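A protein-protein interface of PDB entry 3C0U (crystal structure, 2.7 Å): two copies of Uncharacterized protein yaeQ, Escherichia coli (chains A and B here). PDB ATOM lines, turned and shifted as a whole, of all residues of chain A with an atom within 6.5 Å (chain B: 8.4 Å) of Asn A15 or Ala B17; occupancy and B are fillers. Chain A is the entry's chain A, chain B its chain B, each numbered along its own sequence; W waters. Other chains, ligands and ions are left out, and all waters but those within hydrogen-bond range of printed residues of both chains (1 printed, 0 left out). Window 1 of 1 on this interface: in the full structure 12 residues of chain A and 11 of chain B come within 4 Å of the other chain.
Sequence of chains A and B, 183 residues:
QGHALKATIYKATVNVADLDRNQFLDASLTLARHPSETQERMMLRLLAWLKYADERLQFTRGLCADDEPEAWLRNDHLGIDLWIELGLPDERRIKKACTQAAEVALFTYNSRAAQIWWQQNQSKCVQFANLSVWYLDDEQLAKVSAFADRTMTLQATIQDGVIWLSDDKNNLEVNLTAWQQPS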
ATOM      1  N   THR A  13       8.252   9.193  10.376  1.00  0.00           N
ATOM      2  CA  THR A  13       9.643   9.373  10.056  1.00  0.00           C
ATOM      3  C   THR A  13      10.256   8.017  10.341  1.00  0.00           C
ATOM      4  O   THR A  13      10.201   7.531  11.474  1.00  0.00           O
ATOM      5  CB  THR A  13      10.281  10.419  10.968  1.00  0.00           C
ATOM      6  OG1 THR A  13       9.409  11.541  11.063  1.00  0.00           O
ATOM      7  CG2 THR A  13      11.593  10.882  10.408  1.00  0.00           C
ATOM      8  N   VAL A  14      10.827   7.401   9.318  1.00  0.00           N
ATOM      9  CA  VAL A  14      11.366   6.066   9.455  1.00  0.00           C
ATOM     10  C   VAL A  14      12.843   5.991   9.075  1.00  0.00           C
ATOM     11  O   VAL A  14      13.290   6.636   8.112  1.00  0.00           O
ATOM     12  CB  VAL A  14      10.560   5.073   8.605  1.00  0.00           C
ATOM     13  CG1 VAL A  14       9.115   5.025   9.087  1.00  0.00           C
ATOM     14  CG2 VAL A  14      10.635   5.431   7.116  1.00  0.00           C
ATOM     15  N   ASN A  15      13.603   5.214   9.840  1.00  0.00           N
ATOM     16  CA  ASN A  15      14.955   4.832   9.448  1.00  0.00           C
ATOM     17  C   ASN A  15      14.987   3.324   9.293  1.00  0.00           C
ATOM     18  O   ASN A  15      14.546   2.596  10.184  1.00  0.00           O
ATOM     19  CB  ASN A  15      15.999   5.280  10.467  1.00  0.00           C
ATOM     20  CG  ASN A  15      17.415   4.835  10.086  1.00  0.00           C
ATOM     21  OD1 ASN A  15      17.899   3.804  10.554  1.00  0.00           O
ATOM     22  ND2 ASN A  15      18.074   5.606   9.223  1.00  0.00           N
ATOM     23  N   VAL A  16      15.494   2.862   8.154  1.00  0.00           N
ATOM     24  CA  VAL A  16      15.554   1.440   7.862  1.00  0.00           C
ATOM     25  C   VAL A  16      16.992   1.028   7.613  1.00  0.00           C
ATOM     26  O   VAL A  16      17.668   1.584   6.754  1.00  0.00           O
ATOM     27  CB  VAL A  16      14.699   1.063   6.616  1.00  0.00           C
ATOM     28  CG1 VAL A  16      14.862  -0.425   6.269  1.00  0.00           C
ATOM     29  CG2 VAL A  16      13.237   1.429   6.828  1.00  0.00           C
ATOM     30  N   ALA A  17      17.460   0.057   8.376  1.00  0.00           N
ATOM     31  CA  ALA A  17      18.732  -0.563   8.095  1.00  0.00           C
ATOM     32  C   ALA A  17      18.491  -2.039   7.792  1.00  0.00           C
ATOM     33  O   ALA A  17      18.272  -2.848   8.700  1.00  0.00           O
ATOM     34  CB  ALA A  17      19.683  -0.377   9.266  1.00  0.00           C
ATOM     35  N   PHE A  24      20.062   1.073   3.239  1.00  0.00           N
ATOM     36  CA  PHE A  24      19.997   2.055   4.313  1.00  0.00           C
ATOM     37  C   PHE A  24      19.270   3.272   3.806  1.00  0.00           C
ATOM     38  O   PHE A  24      19.629   3.839   2.774  1.00  0.00           O
ATOM     39  CB  PHE A  24      21.394   2.396   4.809  1.00  0.00           C
ATOM     40  CG  PHE A  24      22.158   1.200   5.276  1.00  0.00           C
ATOM     41  CD1 PHE A  24      23.015   0.526   4.411  1.00  0.00           C
ATOM     42  CD2 PHE A  24      22.000   0.724   6.579  1.00  0.00           C
ATOM     43  CE1 PHE A  24      23.720  -0.596   4.840  1.00  0.00           C
ATOM     44  CE2 PHE A  24      22.696  -0.395   7.020  1.00  0.00           C
ATOM     45  CZ  PHE A  24      23.563  -1.057   6.149  1.00  0.00           C
ATOM     46  N   LEU A  25      18.229   3.659   4.529  1.00  0.00           N
ATOM     47  CA  LEU A  25      17.314   4.657   4.038  1.00  0.00           C
ATOM     48  C   LEU A  25      16.616   5.426   5.154  1.00  0.00           C
ATOM     49  O   LEU A  25      16.311   4.878   6.224  1.00  0.00           O
ATOM     50  CB  LEU A  25      16.309   3.969   3.106  1.00  0.00           C
ATOM     51  CG  LEU A  25      14.921   4.516   2.787  1.00  0.00           C
ATOM     52  CD1 LEU A  25      14.504   4.022   1.432  1.00  0.00           C
ATOM     53  CD2 LEU A  25      13.917   4.078   3.854  1.00  0.00           C
ATOM     54  N   ASP A  26      16.406   6.715   4.886  1.00  0.00           N
ATOM     55  CA  ASP A  26      15.541   7.578   5.672  1.00  0.00           C
ATOM     56  C   ASP A  26      14.395   7.988   4.800  1.00  0.00           C
ATOM     57  O   ASP A  26      14.595   8.290   3.629  1.00  0.00           O
ATOM     58  CB  ASP A  26      16.277   8.834   6.084  1.00  0.00           C
ATOM     59  CG  ASP A  26      17.200   8.599   7.231  1.00  0.00           C
ATOM     60  OD1 ASP A  26      18.422   8.807   7.062  1.00  0.00           O
ATOM     61  OD2 ASP A  26      16.703   8.197   8.306  1.00  0.00           O
ATOM     62  N   ALA A  27      13.193   8.010   5.363  1.00  0.00           N
ATOM     63  CA  ALA A  27      12.026   8.443   4.612  1.00  0.00           C
ATOM     64  C   ALA A  27      11.012   9.036   5.555  1.00  0.00           C
ATOM     65  O   ALA A  27      10.965   8.683   6.734  1.00  0.00           O
ATOM     66  CB  ALA A  27      11.413   7.276   3.849  1.00  0.00           C
ATOM     67  N   LEU A  50       8.231  -1.155   5.174  1.00  0.00           N
ATOM     68  CA  LEU A  50       9.537  -1.252   5.815  1.00  0.00           C
ATOM     69  C   LEU A  50      10.317  -2.460   5.282  1.00  0.00           C
ATOM     70  O   LEU A  50      11.539  -2.392   5.071  1.00  0.00           O
ATOM     71  CB  LEU A  50       9.407  -1.326   7.349  1.00  0.00           C
ATOM     72  CG  LEU A  50       8.777  -0.155   8.111  1.00  0.00           C
ATOM     73  CD1 LEU A  50       8.579  -0.540   9.543  1.00  0.00           C
ATOM     74  CD2 LEU A  50       9.600   1.137   8.011  1.00  0.00           C
ATOM     75  N   LEU A 154      10.077   5.941  13.850  1.00  0.00           N
ATOM     76  CA  LEU A 154      10.435   4.530  13.913  1.00  0.00           C
ATOM     77  C   LEU A 154      11.816   4.248  13.330  1.00  0.00           C
ATOM     78  O   LEU A 154      12.328   5.000  12.496  1.00  0.00           O
ATOM     79  CB  LEU A 154       9.381   3.678  13.185  1.00  0.00           C
ATOM     80  CG  LEU A 154       7.903   3.799  13.597  1.00  0.00           C
ATOM     81  CD1 LEU A 154       7.006   3.163  12.567  1.00  0.00           C
ATOM     82  CD2 LEU A 154       7.658   3.182  14.957  1.00  0.00           C
ATOM     83  N   GLN A 155      12.419   3.163  13.798  1.00  0.00           N
ATOM     84  CA  GLN A 155      13.626   2.629  13.196  1.00  0.00           C
ATOM     85  C   GLN A 155      13.438   1.128  13.050  1.00  0.00           C
ATOM     86  O   GLN A 155      12.937   0.456  13.953  1.00  0.00           O
ATOM     87  CB  GLN A 155      14.879   3.020  14.003  1.00  0.00           C
ATOM     88  CG  GLN A 155      15.828   1.879  14.408  1.00  0.00           C
ATOM     89  CD  GLN A 155      16.651   1.302  13.271  1.00  0.00           C
ATOM     90  OE1 GLN A 155      16.999   0.125  13.288  1.00  0.00           O
ATOM     91  NE2 GLN A 155      16.970   2.122  12.283  1.00  0.00           N
ATOM     92  N   ALA A 156      13.817   0.618  11.889  1.00  0.00           N
ATOM     93  CA  ALA A 156      13.685  -0.790  11.596  1.00  0.00           C
ATOM     94  C   ALA A 156      15.024  -1.355  11.156  1.00  0.00           C
ATOM     95  O   ALA A 156      15.614  -0.889  10.179  1.00  0.00           O
ATOM     96  CB  ALA A 156      12.623  -1.006  10.519  1.00  0.00           C
ATOM     97  N   THR A 157      15.509  -2.344  11.898  1.00  0.00           N
ATOM     98  CA  THR A 157      16.688  -3.112  11.498  1.00  0.00           C
ATOM     99  C   THR A 157      16.273  -4.511  11.046  1.00  0.00           C
ATOM    100  O   THR A 157      15.543  -5.216  11.745  1.00  0.00           O
ATOM    101  CB  THR A 157      17.756  -3.189  12.616  1.00  0.00           C
ATOM    102  OG1 THR A 157      17.301  -2.458  13.754  1.00  0.00           O
ATOM    103  CG2 THR A 157      19.048  -2.563  12.167  1.00  0.00           C
ATOM    104  N   VAL B  14      28.170   8.724   8.102  1.00  0.00           N
ATOM    105  CA  VAL B  14      27.540   8.194   9.272  1.00  0.00           C
ATOM    106  C   VAL B  14      26.057   8.532   9.263  1.00  0.00           C
ATOM    107  O   VAL B  14      25.674   9.663   8.952  1.00  0.00           O
ATOM    108  CB  VAL B  14      28.254   8.721  10.519  1.00  0.00           C
ATOM    109  CG1 VAL B  14      27.774  10.154  10.892  1.00  0.00           C
ATOM    110  CG2 VAL B  14      28.089   7.746  11.646  1.00  0.00           C
ATOM    111  N   ASN B  15      25.222   7.540   9.549  1.00  0.00           N
ATOM    112  CA  ASN B  15      23.803   7.796   9.763  1.00  0.00           C
ATOM    113  C   ASN B  15      23.435   7.433  11.186  1.00  0.00           C
ATOM    114  O   ASN B  15      23.741   6.324  11.663  1.00  0.00           O
ATOM    115  CB  ASN B  15      22.904   7.034   8.777  1.00  0.00           C
ATOM    116  CG  ASN B  15      21.414   7.337   8.996  1.00  0.00           C
ATOM    117  OD1 ASN B  15      20.745   6.665   9.790  1.00  0.00           O
ATOM    118  ND2 ASN B  15      20.901   8.379   8.327  1.00  0.00           N
ATOM    119  N   VAL B  16      22.771   8.364  11.856  1.00  0.00           N
ATOM    120  CA  VAL B  16      22.441   8.184  13.260  1.00  0.00           C
ATOM    121  C   VAL B  16      20.935   8.216  13.436  1.00  0.00           C
ATOM    122  O   VAL B  16      20.273   9.188  13.052  1.00  0.00           O
ATOM    123  CB  VAL B  16      23.118   9.264  14.158  1.00  0.00           C
ATOM    124  CG1 VAL B  16      22.777   9.043  15.639  1.00  0.00           C
ATOM    125  CG2 VAL B  16      24.623   9.268  13.956  1.00  0.00           C
ATOM    126  N   ALA B  17      20.400   7.145  14.007  1.00  0.00           N
ATOM    127  CA  ALA B  17      18.988   7.099  14.358  1.00  0.00           C
ATOM    128  C   ALA B  17      18.875   7.129  15.877  1.00  0.00           C
ATOM    129  O   ALA B  17      18.931   6.084  16.542  1.00  0.00           O
ATOM    130  CB  ALA B  17      18.307   5.856  13.764  1.00  0.00           C
ATOM    131  N   ASP B  18      18.738   8.338  16.418  1.00  0.00           N
ATOM    132  CA  ASP B  18      18.668   8.520  17.853  1.00  0.00           C
ATOM    133  C   ASP B  18      17.234   8.579  18.375  1.00  0.00           C
ATOM    134  O   ASP B  18      16.574   9.614  18.292  1.00  0.00           O
ATOM    135  CB  ASP B  18      19.421   9.776  18.256  1.00  0.00           C
ATOM    136  CG  ASP B  18      19.667   9.857  19.749  1.00  0.00           C
ATOM    137  OD1 ASP B  18      18.846   9.337  20.544  1.00  0.00           O
ATOM    138  OD2 ASP B  18      20.702  10.454  20.128  1.00  0.00           O
ATOM    139  N   LEU B  19      16.772   7.475  18.948  1.00  0.00           N
ATOM    140  CA  LEU B  19      15.418   7.405  19.474  1.00  0.00           C
ATOM    141  C   LEU B  19      15.269   8.103  20.829  1.00  0.00           C
ATOM    142  O   LEU B  19      14.191   8.601  21.143  1.00  0.00           O
ATOM    143  CB  LEU B  19      14.928   5.959  19.527  1.00  0.00           C
ATOM    144  CG  LEU B  19      14.804   5.275  18.158  1.00  0.00           C
ATOM    145  CD1 LEU B  19      15.040   3.780  18.255  1.00  0.00           C
ATOM    146  CD2 LEU B  19      13.463   5.570  17.481  1.00  0.00           C
ATOM    147  N   ASP B  20      16.340   8.155  21.623  1.00  0.00           N
ATOM    148  CA  ASP B  20      16.314   8.887  22.895  1.00  0.00           C
ATOM    149  C   ASP B  20      16.054  10.382  22.696  1.00  0.00           C
ATOM    150  O   ASP B  20      15.296  10.973  23.448  1.00  0.00           O
ATOM    151  CB  ASP B  20      17.614   8.702  23.686  1.00  0.00           C
ATOM    152  CG  ASP B  20      17.816   7.277  24.182  1.00  0.00           C
ATOM    153  OD1 ASP B  20      16.836   6.503  24.236  1.00  0.00           O
ATOM    154  OD2 ASP B  20      18.971   6.924  24.522  1.00  0.00           O
ATOM    155  N   ARG B  21      16.679  10.984  21.685  1.00  0.00           N
ATOM    156  CA  ARG B  21      16.606  12.434  21.466  1.00  0.00           C
ATOM    157  C   ARG B  21      15.697  12.814  20.290  1.00  0.00           C
ATOM    158  O   ARG B  21      15.633  13.983  19.897  1.00  0.00           O
ATOM    159  CB  ARG B  21      18.012  12.995  21.242  1.00  0.00           C
ATOM    160  CG  ARG B  21      18.960  12.878  22.446  1.00  0.00           C
ATOM    161  CD  ARG B  21      20.435  12.814  22.008  1.00  0.00           C
ATOM    162  NE  ARG B  21      20.835  13.991  21.242  1.00  0.00           N
ATOM    163  CZ  ARG B  21      21.773  14.012  20.298  1.00  0.00           C
ATOM    164  NH1 ARG B  21      22.439  12.916  19.966  1.00  0.00           N
ATOM    165  NH2 ARG B  21      22.034  15.146  19.670  1.00  0.00           N
ATOM    166  N   ASN B  22      14.987  11.821  19.742  1.00  0.00           N
ATOM    167  CA  ASN B  22      14.147  11.988  18.543  1.00  0.00           C
ATOM    168  C   ASN B  22      14.860  12.756  17.413  1.00  0.00           C
ATOM    169  O   ASN B  22      14.376  13.776  16.908  1.00  0.00           O
ATOM    170  CB  ASN B  22      12.803  12.635  18.901  1.00  0.00           C
ATOM    171  CG  ASN B  22      11.788  12.531  17.778  1.00  0.00           C
ATOM    172  OD1 ASN B  22      11.746  11.534  17.067  1.00  0.00           O
ATOM    173  ND2 ASN B  22      10.974  13.564  17.610  1.00  0.00           N
ATOM    174  N   GLN B  23      16.031  12.258  17.036  1.00  0.00           N
ATOM    175  CA  GLN B  23      16.845  12.922  16.039  1.00  0.00           C
ATOM    176  C   GLN B  23      17.487  11.950  15.064  1.00  0.00           C
ATOM    177  O   GLN B  23      18.277  11.084  15.454  1.00  0.00           O
ATOM    178  CB  GLN B  23      17.929  13.764  16.698  1.00  0.00           C
ATOM    179  CG  GLN B  23      18.975  14.268  15.710  1.00  0.00           C
ATOM    180  CD  GLN B  23      19.981  15.175  16.362  1.00  0.00           C
ATOM    181  OE1 GLN B  23      19.615  16.067  17.127  1.00  0.00           O
ATOM    182  NE2 GLN B  23      21.260  14.949  16.078  1.00  0.00           N
ATOM    183  N   PHE B  24      17.143  12.114  13.794  1.00  0.00           N
ATOM    184  CA  PHE B  24      17.762  11.354  12.730  1.00  0.00           C
ATOM    185  C   PHE B  24      18.704  12.276  11.948  1.00  0.00           C
ATOM    186  O   PHE B  24      18.326  13.381  11.562  1.00  0.00           O
ATOM    187  CB  PHE B  24      16.676  10.721  11.847  1.00  0.00           C
ATOM    188  CG  PHE B  24      15.902   9.610  12.531  1.00  0.00           C
ATOM    189  CD1 PHE B  24      16.076   9.336  13.893  1.00  0.00           C
ATOM    190  CD2 PHE B  24      14.984   8.851  11.820  1.00  0.00           C
ATOM    191  CE1 PHE B  24      15.361   8.316  14.526  1.00  0.00           C
ATOM    192  CE2 PHE B  24      14.255   7.827  12.448  1.00  0.00           C
ATOM    193  CZ  PHE B  24      14.452   7.560  13.801  1.00  0.00           C
ATOM    194  N   LEU B  25      19.935  11.830  11.726  1.00  0.00           N
ATOM    195  CA  LEU B  25      20.942  12.694  11.129  1.00  0.00           C
ATOM    196  C   LEU B  25      21.875  11.929  10.187  1.00  0.00           C
ATOM    197  O   LEU B  25      22.207  10.766  10.437  1.00  0.00           O
ATOM    198  CB  LEU B  25      21.711  13.393  12.263  1.00  0.00           C
ATOM    199  CG  LEU B  25      22.975  14.239  12.118  1.00  0.00           C
ATOM    200  CD1 LEU B  25      23.202  14.992  13.392  1.00  0.00           C
ATOM    201  CD2 LEU B  25      24.188  13.378  11.844  1.00  0.00           C
ATOM    202  N   ASP B  26      22.272  12.594   9.098  1.00  0.00           N
ATOM    203  CA  ASP B  26      23.346  12.142   8.194  1.00  0.00           C
ATOM    204  C   ASP B  26      24.509  13.113   8.250  1.00  0.00           C
ATOM    205  O   ASP B  26      24.304  14.323   8.231  1.00  0.00           O
ATOM    206  CB  ASP B  26      22.856  12.097   6.749  1.00  0.00           C
ATOM    207  CG  ASP B  26      21.950  10.916   6.472  1.00  0.00           C
ATOM    208  OD1 ASP B  26      22.347   9.760   6.757  1.00  0.00           O
ATOM    209  OD2 ASP B  26      20.837  11.141   5.944  1.00  0.00           O
ATOM    210  N   LEU B  50      28.975  10.179  17.669  1.00  0.00           N
ATOM    211  CA  LEU B  50      27.665   9.545  17.487  1.00  0.00           C
ATOM    212  C   LEU B  50      26.693   9.824  18.657  1.00  0.00           C
ATOM    213  O   LEU B  50      25.532  10.214  18.436  1.00  0.00           O
ATOM    214  CB  LEU B  50      27.790   8.030  17.222  1.00  0.00           C
ATOM    215  CG  LEU B  50      28.642   7.555  16.035  1.00  0.00           C
ATOM    216  CD1 LEU B  50      28.700   6.047  15.987  1.00  0.00           C
ATOM    217  CD2 LEU B  50      28.134   8.093  14.715  1.00  0.00           C
ATOM    218  N   ALA B  53      25.687  13.453  18.452  1.00  0.00           N
ATOM    219  CA  ALA B  53      25.592  13.862  17.058  1.00  0.00           C
ATOM    220  C   ALA B  53      24.836  15.164  16.885  1.00  0.00           C
ATOM    221  O   ALA B  53      23.748  15.347  17.447  1.00  0.00           O
ATOM    222  CB  ALA B  53      24.956  12.773  16.237  1.00  0.00           C
ATOM    223  N   LEU B 154      28.927   3.995   8.342  1.00  0.00           N
ATOM    224  CA  LEU B 154      28.388   3.537   9.609  1.00  0.00           C
ATOM    225  C   LEU B 154      26.921   3.873   9.807  1.00  0.00           C
ATOM    226  O   LEU B 154      26.445   4.948   9.424  1.00  0.00           O
ATOM    227  CB  LEU B 154      29.219   4.082  10.774  1.00  0.00           C
ATOM    228  CG  LEU B 154      30.709   3.739  10.806  1.00  0.00           C
ATOM    229  CD1 LEU B 154      31.382   4.487  11.952  1.00  0.00           C
ATOM    230  CD2 LEU B 154      30.953   2.241  10.925  1.00  0.00           C
ATOM    231  N   GLN B 155      26.223   2.931  10.429  1.00  0.00           N
ATOM    232  CA  GLN B 155      24.867   3.131  10.914  1.00  0.00           C
ATOM    233  C   GLN B 155      24.872   3.003  12.439  1.00  0.00           C
ATOM    234  O   GLN B 155      25.505   2.093  12.966  1.00  0.00           O
ATOM    235  CB  GLN B 155      23.941   2.087  10.278  1.00  0.00           C
ATOM    236  CG  GLN B 155      22.659   1.784  11.070  1.00  0.00           C
ATOM    237  CD  GLN B 155      21.719   2.956  11.096  1.00  0.00           C
ATOM    238  OE1 GLN B 155      21.655   3.721  10.136  1.00  0.00           O
ATOM    239  NE2 GLN B 155      20.991   3.118  12.194  1.00  0.00           N
ATOM    240  N   ALA B 156      24.186   3.916  13.133  1.00  0.00           N
ATOM    241  CA  ALA B 156      24.013   3.843  14.598  1.00  0.00           C
ATOM    242  C   ALA B 156      22.581   4.105  15.047  1.00  0.00           C
ATOM    243  O   ALA B 156      21.974   5.115  14.679  1.00  0.00           O
ATOM    244  CB  ALA B 156      24.948   4.806  15.303  1.00  0.00           C
ATOM    245  N   THR B 157      22.048   3.199  15.854  1.00  0.00           N
ATOM    246  CA  THR B 157      20.748   3.393  16.470  1.00  0.00           C
ATOM    247  C   THR B 157      20.947   3.573  17.962  1.00  0.00           C
ATOM    248  O   THR B 157      21.700   2.825  18.582  1.00  0.00           O
ATOM    249  CB  THR B 157      19.798   2.216  16.187  1.00  0.00           C
ATOM    250  OG1 THR B 157      19.529   2.153  14.782  1.00  0.00           O
ATOM    251  CG2 THR B 157      18.473   2.375  16.938  1.00  0.00           C
ATOM    252  N   ILE B 158      20.297   4.581  18.533  1.00  0.00           N
ATOM    253  CA  ILE B 158      20.402   4.830  19.962  1.00  0.00           C
ATOM    254  C   ILE B 158      19.033   4.727  20.616  1.00  0.00           C
ATOM    255  O   ILE B 158      18.077   5.375  20.187  1.00  0.00           O
ATOM    256  CB  ILE B 158      21.063   6.202  20.258  1.00  0.00           C
ATOM    257  CG1 ILE B 158      22.509   6.199  19.757  1.00  0.00           C
ATOM    258  CG2 ILE B 158      20.988   6.546  21.757  1.00  0.00           C
ATOM    259  CD1 ILE B 158      23.153   7.562  19.700  1.00  0.00           C
ATOM    260  N   GLN B 159      18.955   3.887  21.644  1.00  0.00           N
ATOM    261  CA  GLN B 159      17.771   3.765  22.484  1.00  0.00           C
ATOM    262  C   GLN B 159      18.222   3.264  23.838  1.00  0.00           C
ATOM    263  O   GLN B 159      18.971   2.276  23.921  1.00  0.00           O
ATOM    264  CB  GLN B 159      16.743   2.793  21.891  1.00  0.00           C
ATOM    265  CG  GLN B 159      15.405   2.801  22.626  1.00  0.00           C
ATOM    266  CD  GLN B 159      14.534   1.618  22.284  1.00  0.00           C
ATOM    267  OE1 GLN B 159      15.018   0.504  22.112  1.00  0.00           O
ATOM    268  NE2 GLN B 159      13.235   1.852  22.196  1.00  0.00           N
ATOM    269  N   VAL B 162      21.885   2.731  24.906  1.00  0.00           N
ATOM    270  CA  VAL B 162      22.562   1.705  24.120  1.00  0.00           C
ATOM    271  C   VAL B 162      22.735   2.190  22.680  1.00  0.00           C
ATOM    272  O   VAL B 162      21.855   2.850  22.126  1.00  0.00           O
ATOM    273  CB  VAL B 162      21.795   0.375  24.148  1.00  0.00           C
ATOM    274  CG1 VAL B 162      22.608  -0.728  23.499  1.00  0.00           C
ATOM    275  CG2 VAL B 162      21.441   0.001  25.583  1.00  0.00           C
ATOM    276  N   ILE B 163      23.888   1.880  22.096  1.00  0.00           N
ATOM    277  CA  ILE B 163      24.202   2.243  20.718  1.00  0.00           C
ATOM    278  C   ILE B 163      24.410   0.975  19.898  1.00  0.00           C
ATOM    279  O   ILE B 163      25.393   0.259  20.091  1.00  0.00           O
ATOM    280  CB  ILE B 163      25.481   3.113  20.639  1.00  0.00           C
ATOM    281  CG1 ILE B 163      25.332   4.390  21.478  1.00  0.00           C
ATOM    282  CG2 ILE B 163      25.835   3.439  19.182  1.00  0.00           C
ATOM    283  CD1 ILE B 163      26.652   5.101  21.784  1.00  0.00           C
ATOM    284  N   TRP B 164      23.472   0.678  19.005  1.00  0.00           N
ATOM    285  CA  TRP B 164      23.690  -0.380  18.024  1.00  0.00           C
ATOM    286  C   TRP B 164      24.464   0.197  16.845  1.00  0.00           C
ATOM    287  O   TRP B 164      23.970   1.048  16.112  1.00  0.00           O
ATOM    288  CB  TRP B 164      22.386  -1.060  17.598  1.00  0.00           C
ATOM    289  CG  TRP B 164      21.951  -2.145  18.559  1.00  0.00           C
ATOM    290  CD1 TRP B 164      22.323  -3.479  18.544  1.00  0.00           C
ATOM    291  CD2 TRP B 164      21.076  -1.991  19.681  1.00  0.00           C
ATOM    292  NE1 TRP B 164      21.723  -4.155  19.591  1.00  0.00           N
ATOM    293  CE2 TRP B 164      20.958  -3.268  20.305  1.00  0.00           C
ATOM    294  CE3 TRP B 164      20.380  -0.901  20.223  1.00  0.00           C
ATOM    295  CZ2 TRP B 164      20.162  -3.480  21.436  1.00  0.00           C
ATOM    296  CZ3 TRP B 164      19.584  -1.109  21.353  1.00  0.00           C
ATOM    297  CH2 TRP B 164      19.482  -2.394  21.948  1.00  0.00           C
HETATM  298  O   HOH W   1      18.429  12.098   7.664  1.00  0.00           O
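The side-chain carboxylate of Asp A26 lies within hydrogen-bond range of the side-chain amide nitrogen of Asn B15, at 2.8 Å.
OD1 of Asn B15 sits at hydrogen-bond distance from ND2 of Asn A15 (2.9 Å).
The side-chain amide oxygen (OE1) of Gln A155 lies within hydrogen-bond range of the side-chain hydroxyl (OG1) of Thr A157.
N of Asn B15 sits at hydrogen-bond distance from O of Leu B154 (2.9 Å).
The side-chain amide oxygen of Gln B155 sits close to the side-chain amide oxygen of Asn B15.
The backbone NH (N) of Leu A154 sits at hydrogen-bond distance from the backbone carbonyl oxygen (O) of Thr A13 (2.9 Å).
The backbone NH (N) of Trp B164 is in hydrogen-bond range of the backbone carbonyl oxygen (O) of Thr B157 (2.8 Å).
N of Ala B17 sits at hydrogen-bond distance from O of Ala B156, 2.7 Å away.
Among the printed residues, merely in contact across the chains: Asn A15 with Ala B17 (3.8 Å), Asn A15 with Phe B24 (3.7 Å), Asn A15 with Gln B155 (3.6 Å), Asp A26 with Phe B24 (3.97 Å), Asp A26 with Asp B26 (3.5 Å), Leu A154 with Phe B24 (3.4 Å) and Gln A155 with Thr B157 (3.4 Å).
Asn A15 touches just these residues of chain B: Asn B15, Ala B17, Phe B24 and Gln B155.
Of chain A, only Asn A15 (3.8 Å) comes within 4 Å of Ala B17.
No residue of chain B comes within 4 Å of Ala A156.
Of the printed residues of chain A, Asp B26 touches Asp A26.
Printed residues of chain A within 4 Å of Phe B24: Asn A15, Asp A26 and Leu A154.
Printed residues of chain B within 4 Å of Gln A155: Thr B157 (3.4 Å).
Val A16 touches none of the printed residues of chain B.
Arg B21 touches none of the printed residues of chain A.
The nearest residue of chain B that does not touch Asn A15 is Thr B157 (4.8 Å).
The nearest printed residue of chain A that does not touch Phe B24 is Val A14 (4.1 Å).
Hydrophobic or aromatic side chains of chain B that line the printed part of chain A: Ala B17 and Phe B24.
Asn B15 touches its own counterpart, Asn A15.
Asn A15 touches Ala B17, but with the chains exchanged Ala A17 does not touch Asn B15 (7.1 Å).
Asp A26 touches Phe B24, but with the chains exchanged Phe A24 does not touch Asp B26 (7.6 Å).
Gln A155 touches Thr B157, but with the chains exchanged Thr A157 does not touch Gln B155 (5.8 Å).
12 positions are printed for both chains.
Of the 9 pairs that touch across the chains among the printed residues, 2 have their exchanged pair printed and touching as well.
Water W1 bridges OD2 of Asp B26 (3.1 Å) and OD1 of Asp A26 (3.3 Å).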
